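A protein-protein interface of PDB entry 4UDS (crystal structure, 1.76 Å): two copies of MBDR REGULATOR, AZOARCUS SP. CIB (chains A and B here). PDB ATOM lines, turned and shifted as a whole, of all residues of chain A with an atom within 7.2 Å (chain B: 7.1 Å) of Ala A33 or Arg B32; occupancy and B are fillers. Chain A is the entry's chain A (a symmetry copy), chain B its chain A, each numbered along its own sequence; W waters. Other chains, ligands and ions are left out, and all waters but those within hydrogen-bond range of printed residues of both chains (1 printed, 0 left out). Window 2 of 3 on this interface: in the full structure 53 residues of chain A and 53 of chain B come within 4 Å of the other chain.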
ATOM      1  N   LEU A  25     -17.044 -17.073 -10.682  1.00  0.00           N
ATOM      2  CA  LEU A  25     -18.141 -16.480  -9.979  1.00  0.00           C
ATOM      3  C   LEU A  25     -19.058 -17.494  -9.220  1.00  0.00           C
ATOM      4  O   LEU A  25     -19.515 -17.214  -8.168  1.00  0.00           O
ATOM      5  CB  LEU A  25     -18.961 -15.592 -10.934  1.00  0.00           C
ATOM      6  CG  LEU A  25     -18.247 -14.366 -11.421  1.00  0.00           C
ATOM      7  CD1 LEU A  25     -18.976 -13.692 -12.568  1.00  0.00           C
ATOM      8  CD2 LEU A  25     -18.182 -13.472 -10.229  1.00  0.00           C
ATOM      9  N   PHE A  26     -19.356 -18.625  -9.838  1.00  0.00           N
ATOM     10  CA  PHE A  26     -20.215 -19.585  -9.184  1.00  0.00           C
ATOM     11  C   PHE A  26     -19.537 -20.044  -7.898  1.00  0.00           C
ATOM     12  O   PHE A  26     -20.160 -20.183  -6.933  1.00  0.00           O
ATOM     13  CB  PHE A  26     -20.439 -20.827 -10.051  1.00  0.00           C
ATOM     14  CG  PHE A  26     -21.295 -20.607 -11.259  1.00  0.00           C
ATOM     15  CD1 PHE A  26     -22.173 -19.571 -11.331  1.00  0.00           C
ATOM     16  CD2 PHE A  26     -21.220 -21.463 -12.321  1.00  0.00           C
ATOM     17  CE1 PHE A  26     -22.990 -19.394 -12.419  1.00  0.00           C
ATOM     18  CE2 PHE A  26     -22.035 -21.296 -13.419  1.00  0.00           C
ATOM     19  CZ  PHE A  26     -22.916 -20.263 -13.471  1.00  0.00           C
ATOM     20  N   ASN A  29     -19.550 -17.007  -5.323  1.00  0.00           N
ATOM     21  CA  ASN A  29     -20.834 -16.470  -4.941  1.00  0.00           C
ATOM     22  C   ASN A  29     -21.975 -17.467  -4.760  1.00  0.00           C
ATOM     23  O   ASN A  29     -22.963 -17.146  -4.203  1.00  0.00           O
ATOM     24  CB  ASN A  29     -21.238 -15.369  -5.936  1.00  0.00           C
ATOM     25  CG  ASN A  29     -20.292 -14.215  -5.911  1.00  0.00           C
ATOM     26  OD1 ASN A  29     -19.419 -14.062  -6.760  1.00  0.00           O
ATOM     27  ND2 ASN A  29     -20.455 -13.394  -4.925  1.00  0.00           N
ATOM     28  N   GLY A  30     -21.820 -18.660  -5.277  1.00  0.00           N
ATOM     29  CA  GLY A  30     -22.910 -19.591  -5.453  1.00  0.00           C
ATOM     30  C   GLY A  30     -23.603 -19.464  -6.807  1.00  0.00           C
ATOM     31  O   GLY A  30     -23.444 -18.480  -7.474  1.00  0.00           O
ATOM     32  N   TYR A  31     -24.355 -20.473  -7.213  1.00  0.00           N
ATOM     33  CA  TYR A  31     -25.042 -20.412  -8.474  1.00  0.00           C
ATOM     34  C   TYR A  31     -26.160 -19.369  -8.558  1.00  0.00           C
ATOM     35  O   TYR A  31     -26.348 -18.732  -9.560  1.00  0.00           O
ATOM     36  CB  TYR A  31     -25.599 -21.793  -8.819  1.00  0.00           C
ATOM     37  CG  TYR A  31     -26.451 -21.916 -10.038  1.00  0.00           C
ATOM     38  CD1 TYR A  31     -25.904 -21.989 -11.317  1.00  0.00           C
ATOM     39  CD2 TYR A  31     -27.788 -22.044  -9.919  1.00  0.00           C
ATOM     40  CE1 TYR A  31     -26.697 -22.128 -12.429  1.00  0.00           C
ATOM     41  CE2 TYR A  31     -28.585 -22.182 -11.004  1.00  0.00           C
ATOM     42  CZ  TYR A  31     -28.051 -22.250 -12.263  1.00  0.00           C
ATOM     43  OH  TYR A  31     -28.973 -22.362 -13.288  1.00  0.00           O
ATOM     44  N   ARG A  32     -26.969 -19.299  -7.525  1.00  0.00           N
ATOM     45  CA  ARG A  32     -28.112 -18.384  -7.577  1.00  0.00           C
ATOM     46  C   ARG A  32     -27.793 -16.896  -7.602  1.00  0.00           C
ATOM     47  O   ARG A  32     -28.408 -16.143  -8.333  1.00  0.00           O
ATOM     48  CB  ARG A  32     -29.153 -18.739  -6.537  1.00  0.00           C
ATOM     49  CG  ARG A  32     -29.586 -20.168  -6.726  1.00  0.00           C
ATOM     50  CD  ARG A  32     -30.815 -20.518  -5.987  1.00  0.00           C
ATOM     51  NE  ARG A  32     -31.938 -19.958  -6.661  1.00  0.00           N
ATOM     52  CZ  ARG A  32     -32.574 -20.569  -7.625  1.00  0.00           C
ATOM     53  NH1 ARG A  32     -32.192 -21.765  -8.044  1.00  0.00           N
ATOM     54  NH2 ARG A  32     -33.574 -19.939  -8.166  1.00  0.00           N
ATOM     55  N   ALA A  33     -26.826 -16.505  -6.793  1.00  0.00           N
ATOM     56  CA  ALA A  33     -26.318 -15.141  -6.771  1.00  0.00           C
ATOM     57  C   ALA A  33     -25.610 -14.719  -8.030  1.00  0.00           C
ATOM     58  O   ALA A  33     -25.418 -13.575  -8.212  1.00  0.00           O
ATOM     59  CB  ALA A  33     -25.403 -14.896  -5.593  1.00  0.00           C
ATOM     60  N   THR A  34     -25.135 -15.650  -8.823  1.00  0.00           N
ATOM     61  CA  THR A  34     -24.421 -15.271 -10.028  1.00  0.00           C
ATOM     62  C   THR A  34     -25.438 -14.986 -11.156  1.00  0.00           C
ATOM     63  O   THR A  34     -26.359 -15.674 -11.295  1.00  0.00           O
ATOM     64  CB  THR A  34     -23.346 -16.328 -10.398  1.00  0.00           C
ATOM     65  OG1 THR A  34     -22.552 -16.658  -9.250  1.00  0.00           O
ATOM     66  CG2 THR A  34     -22.391 -15.832 -11.507  1.00  0.00           C
ATOM     67  N   THR A  35     -25.212 -13.958 -11.938  1.00  0.00           N
ATOM     68  CA  THR A  35     -26.073 -13.592 -13.039  1.00  0.00           C
ATOM     69  C   THR A  35     -25.240 -13.476 -14.308  1.00  0.00           C
ATOM     70  O   THR A  35     -24.108 -13.229 -14.263  1.00  0.00           O
ATOM     71  CB  THR A  35     -26.805 -12.231 -12.826  1.00  0.00           C
ATOM     72  OG1 THR A  35     -25.863 -11.165 -12.791  1.00  0.00           O
ATOM     73  CG2 THR A  35     -27.652 -12.244 -11.564  1.00  0.00           C
ATOM     74  N   MET A  38     -23.351 -10.268 -14.422  1.00  0.00           N
ATOM     75  CA  MET A  38     -22.081 -10.331 -13.719  1.00  0.00           C
ATOM     76  C   MET A  38     -21.014 -11.098 -14.499  1.00  0.00           C
ATOM     77  O   MET A  38     -19.889 -10.699 -14.535  1.00  0.00           O
ATOM     78  CB  MET A  38     -22.285 -10.999 -12.361  1.00  0.00           C
ATOM     79  CG  MET A  38     -23.113 -10.169 -11.392  1.00  0.00           C
ATOM     80  SD  MET A  38     -23.461 -11.024  -9.711  1.00  0.00           S
ATOM     81  CE  MET A  38     -21.667 -10.899  -8.958  1.00  0.00           C
ATOM     82  N   LYS A  57     -27.915 -18.943 -18.082  1.00  0.00           N
ATOM     83  CA  LYS A  57     -27.032 -19.348 -17.015  1.00  0.00           C
ATOM     84  C   LYS A  57     -27.004 -20.864 -16.856  1.00  0.00           C
ATOM     85  O   LYS A  57     -25.946 -21.386 -16.653  1.00  0.00           O
ATOM     86  CB  LYS A  57     -27.437 -18.721 -15.685  1.00  0.00           C
ATOM     87  CG  LYS A  57     -26.333 -18.671 -14.678  1.00  0.00           C
ATOM     88  CD  LYS A  57     -26.743 -17.972 -13.396  1.00  0.00           C
ATOM     89  CE  LYS A  57     -28.058 -18.462 -12.833  1.00  0.00           C
ATOM     90  NZ  LYS A  57     -28.317 -17.893 -11.487  1.00  0.00           N
ATOM     91  N   PHE A 119     -28.520 -28.659  -1.704  1.00  0.00           N
ATOM     92  CA  PHE A 119     -28.158 -27.443  -0.999  1.00  0.00           C
ATOM     93  C   PHE A 119     -27.540 -26.407  -1.906  1.00  0.00           C
ATOM     94  O   PHE A 119     -27.564 -25.248  -1.581  1.00  0.00           O
ATOM     95  CB  PHE A 119     -27.242 -27.743   0.209  1.00  0.00           C
ATOM     96  CG  PHE A 119     -27.033 -26.563   1.130  1.00  0.00           C
ATOM     97  CD1 PHE A 119     -28.086 -25.914   1.707  1.00  0.00           C
ATOM     98  CD2 PHE A 119     -25.785 -26.105   1.406  1.00  0.00           C
ATOM     99  CE1 PHE A 119     -27.892 -24.805   2.520  1.00  0.00           C
ATOM    100  CE2 PHE A 119     -25.577 -25.021   2.217  1.00  0.00           C
ATOM    101  CZ  PHE A 119     -26.642 -24.372   2.773  1.00  0.00           C
ATOM    102  N   PHE B  26     -33.948 -24.746   3.783  1.00  0.00           N
ATOM    103  CA  PHE B  26     -32.615 -24.364   3.377  1.00  0.00           C
ATOM    104  C   PHE B  26     -31.910 -25.593   2.814  1.00  0.00           C
ATOM    105  O   PHE B  26     -31.250 -25.499   1.868  1.00  0.00           O
ATOM    106  CB  PHE B  26     -31.784 -23.862   4.561  1.00  0.00           C
ATOM    107  CG  PHE B  26     -32.200 -22.530   5.104  1.00  0.00           C
ATOM    108  CD1 PHE B  26     -32.901 -21.641   4.351  1.00  0.00           C
ATOM    109  CD2 PHE B  26     -31.867 -22.172   6.379  1.00  0.00           C
ATOM    110  CE1 PHE B  26     -33.243 -20.403   4.831  1.00  0.00           C
ATOM    111  CE2 PHE B  26     -32.206 -20.932   6.875  1.00  0.00           C
ATOM    112  CZ  PHE B  26     -32.895 -20.050   6.104  1.00  0.00           C
ATOM    113  N   ASN B  29     -33.614 -26.535  -0.659  1.00  0.00           N
ATOM    114  CA  ASN B  29     -33.589 -25.535  -1.699  1.00  0.00           C
ATOM    115  C   ASN B  29     -32.326 -24.688  -1.816  1.00  0.00           C
ATOM    116  O   ASN B  29     -32.126 -24.048  -2.785  1.00  0.00           O
ATOM    117  CB  ASN B  29     -34.828 -24.633  -1.563  1.00  0.00           C
ATOM    118  CG  ASN B  29     -36.099 -25.390  -1.759  1.00  0.00           C
ATOM    119  OD1 ASN B  29     -36.796 -25.757  -0.818  1.00  0.00           O
ATOM    120  ND2 ASN B  29     -36.405 -25.638  -2.990  1.00  0.00           N
ATOM    121  N   GLY B  30     -31.510 -24.680  -0.791  1.00  0.00           N
ATOM    122  CA  GLY B  30     -30.453 -23.707  -0.633  1.00  0.00           C
ATOM    123  C   GLY B  30     -30.887 -22.460   0.132  1.00  0.00           C
ATOM    124  O   GLY B  30     -32.053 -22.216   0.272  1.00  0.00           O
ATOM    125  N   TYR B  31     -29.942 -21.686   0.639  1.00  0.00           N
ATOM    126  CA  TYR B  31     -30.284 -20.492   1.361  1.00  0.00           C
ATOM    127  C   TYR B  31     -30.929 -19.384   0.523  1.00  0.00           C
ATOM    128  O   TYR B  31     -31.819 -18.705   0.962  1.00  0.00           O
ATOM    129  CB  TYR B  31     -29.041 -19.948   2.065  1.00  0.00           C
ATOM    130  CG  TYR B  31     -29.159 -18.642   2.777  1.00  0.00           C
ATOM    131  CD1 TYR B  31     -29.730 -18.540   4.043  1.00  0.00           C
ATOM    132  CD2 TYR B  31     -28.632 -17.525   2.234  1.00  0.00           C
ATOM    133  CE1 TYR B  31     -29.810 -17.336   4.699  1.00  0.00           C
ATOM    134  CE2 TYR B  31     -28.701 -16.331   2.866  1.00  0.00           C
ATOM    135  CZ  TYR B  31     -29.265 -16.226   4.109  1.00  0.00           C
ATOM    136  OH  TYR B  31     -29.300 -14.946   4.634  1.00  0.00           O
ATOM    137  N   ARG B  32     -30.376 -19.141  -0.644  1.00  0.00           N
ATOM    138  CA  ARG B  32     -30.889 -18.037  -1.458  1.00  0.00           C
ATOM    139  C   ARG B  32     -32.300 -18.191  -2.005  1.00  0.00           C
ATOM    140  O   ARG B  32     -33.073 -17.251  -1.999  1.00  0.00           O
ATOM    141  CB  ARG B  32     -29.894 -17.626  -2.522  1.00  0.00           C
ATOM    142  CG  ARG B  32     -28.584 -17.267  -1.874  1.00  0.00           C
ATOM    143  CD  ARG B  32     -27.656 -16.550  -2.770  1.00  0.00           C
ATOM    144  NE  ARG B  32     -28.095 -15.202  -2.914  1.00  0.00           N
ATOM    145  CZ  ARG B  32     -27.746 -14.242  -2.099  1.00  0.00           C
ATOM    146  NH1 ARG B  32     -26.953 -14.480  -1.066  1.00  0.00           N
ATOM    147  NH2 ARG B  32     -28.231 -13.060  -2.336  1.00  0.00           N
ATOM    148  N   ALA B  33     -32.607 -19.389  -2.468  1.00  0.00           N
ATOM    149  CA  ALA B  33     -33.943 -19.742  -2.923  1.00  0.00           C
ATOM    150  C   ALA B  33     -34.989 -19.752  -1.841  1.00  0.00           C
ATOM    151  O   ALA B  33     -36.121 -19.749  -2.150  1.00  0.00           O
ATOM    152  CB  ALA B  33     -33.966 -21.075  -3.634  1.00  0.00           C
ATOM    153  N   THR B  34     -34.598 -19.878  -0.595  1.00  0.00           N
ATOM    154  CA  THR B  34     -35.586 -19.922   0.467  1.00  0.00           C
ATOM    155  C   THR B  34     -35.984 -18.480   0.855  1.00  0.00           C
ATOM    156  O   THR B  34     -35.175 -17.656   0.935  1.00  0.00           O
ATOM    157  CB  THR B  34     -35.088 -20.783   1.659  1.00  0.00           C
ATOM    158  OG1 THR B  34     -34.582 -22.041   1.192  1.00  0.00           O
ATOM    159  CG2 THR B  34     -36.211 -21.076   2.681  1.00  0.00           C
ATOM    160  N   THR B  35     -37.251 -18.239   1.092  1.00  0.00           N
ATOM    161  CA  THR B  35     -37.754 -16.941   1.480  1.00  0.00           C
ATOM    162  C   THR B  35     -38.566 -17.082   2.759  1.00  0.00           C
ATOM    163  O   THR B  35     -39.080 -18.084   3.038  1.00  0.00           O
ATOM    164  CB  THR B  35     -38.673 -16.287   0.403  1.00  0.00           C
ATOM    165  OG1 THR B  35     -39.861 -17.052   0.239  1.00  0.00           O
ATOM    166  CG2 THR B  35     -37.950 -16.123  -0.924  1.00  0.00           C
ATOM    167  N   LYS B  57     -34.428 -13.400   7.299  1.00  0.00           N
ATOM    168  CA  LYS B  57     -33.910 -14.704   6.965  1.00  0.00           C
ATOM    169  C   LYS B  57     -32.518 -14.921   7.548  1.00  0.00           C
ATOM    170  O   LYS B  57     -32.272 -15.990   8.028  1.00  0.00           O
ATOM    171  CB  LYS B  57     -33.848 -14.913   5.455  1.00  0.00           C
ATOM    172  CG  LYS B  57     -33.816 -16.349   5.043  1.00  0.00           C
ATOM    173  CD  LYS B  57     -33.835 -16.525   3.537  1.00  0.00           C
ATOM    174  CE  LYS B  57     -32.825 -15.662   2.813  1.00  0.00           C
ATOM    175  NZ  LYS B  57     -32.746 -16.010   1.373  1.00  0.00           N
ATOM    176  N   SER B 120     -21.985 -21.840  -0.768  1.00  0.00           N
ATOM    177  CA  SER B 120     -23.280 -21.943  -0.137  1.00  0.00           C
ATOM    178  C   SER B 120     -24.158 -20.725  -0.320  1.00  0.00           C
ATOM    179  O   SER B 120     -25.348 -20.809  -0.193  1.00  0.00           O
ATOM    180  CB  SER B 120     -23.162 -22.275   1.354  1.00  0.00           C
ATOM    181  OG  SER B 120     -22.495 -21.261   2.044  1.00  0.00           O
ATOM    182  N   GLY B 121     -23.516 -19.616  -0.594  1.00  0.00           N
ATOM    183  CA  GLY B 121     -24.183 -18.378  -0.902  1.00  0.00           C
ATOM    184  C   GLY B 121     -24.837 -17.566   0.185  1.00  0.00           C
ATOM    185  O   GLY B 121     -25.797 -16.899  -0.072  1.00  0.00           O
ATOM    186  N   THR B 122     -24.324 -17.664   1.396  1.00  0.00           N
ATOM    187  CA  THR B 122     -24.884 -16.976   2.555  1.00  0.00           C
ATOM    188  C   THR B 122     -24.317 -15.602   2.853  1.00  0.00           C
ATOM    189  O   THR B 122     -24.877 -14.858   3.610  1.00  0.00           O
ATOM    190  CB  THR B 122     -24.742 -17.806   3.851  1.00  0.00           C
ATOM    191  OG1 THR B 122     -23.371 -17.962   4.210  1.00  0.00           O
ATOM    192  CG2 THR B 122     -25.379 -19.140   3.704  1.00  0.00           C
ATOM    193  N   GLY B 123     -23.155 -15.342   2.321  1.00  0.00           N
ATOM    194  CA  GLY B 123     -22.479 -14.135   2.692  1.00  0.00           C
ATOM    195  C   GLY B 123     -21.586 -14.249   3.944  1.00  0.00           C
ATOM    196  O   GLY B 123     -21.767 -15.075   4.806  1.00  0.00           O
HETATM  197  O   HOH W   1     -27.441 -22.630  -0.433  1.00  0.00           O
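Of chain B, only Arg B32 comes within 4 Å of Ala A33. Of the printed residues of chain B, Arg A32 touches Ala B33 (3.8 Å). Of the printed residues of chain A, Ser B120 touches Phe A119. Of the printed residues of chain B, Asn A29 touches Gly B121 (3.7 Å). Of the printed residues of chain A, Phe B26 touches Phe A119 (3.2 Å). Printed residues of chain B within 4 Å of Phe A119: Phe B26, Gly B30 and Ser B120. Thr B122 touches none of the printed residues of chain A. Tyr A31 touches none of the printed residues of chain B. The nearest residue of chain A that does not touch Arg B32 is Arg A32 (4.2 Å). The nearest printed residue of chain A that does not touch Gly B30 is Arg A32 (6.2 Å).
Arg A32 touches Ala B33, and with the chains exchanged Ala A33 touches Arg B32. Of the 6 pairs that touch across the chains among the printed residues, 2 have their exchanged pair printed and touching as well.
The backbone carbonyl oxygen of Gly B30 is in hydrogen-bond range of the side-chain hydroxyl of Thr B34. NH1 of Arg B32 sits at hydrogen-bond distance from O of Gly B121, 2.9 Å away. The backbone carbonyl oxygen of Leu A25 sits close to the side-chain amide oxygen of Asn A29 (3.5 Å).
Water W1 lies within hydrogen-bond range of O of Ser B120 (2.8 Å), O of Phe A119 (2.9 Å) and N of Tyr B31 (2.9 Å).
Among the printed residues, merely in contact across the chains: Asn A29 with Gly B121, Arg A32 with Ala B33, Ala A33 with Arg B32, Phe A119 with Phe B26, Phe A119 with Gly B30 and Phe A119 with Ser B120.
Of the 12 printed residues of chain A, 4 touch a printed residue of chain B. Hydrophobic or aromatic side chains of chain A within 4 Å of the printed part of chain B: Ala A33 and Phe A119. Printed residues of chain B that touch a printed residue of chain A: Phe B26, Gly B30, Arg B32, Ala B33, Ser B120 and Gly B121. Among the printed residues, no Asp or Glu carboxylate lies within 4 Å of a Lys or Arg side-chain nitrogen of the other chain.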
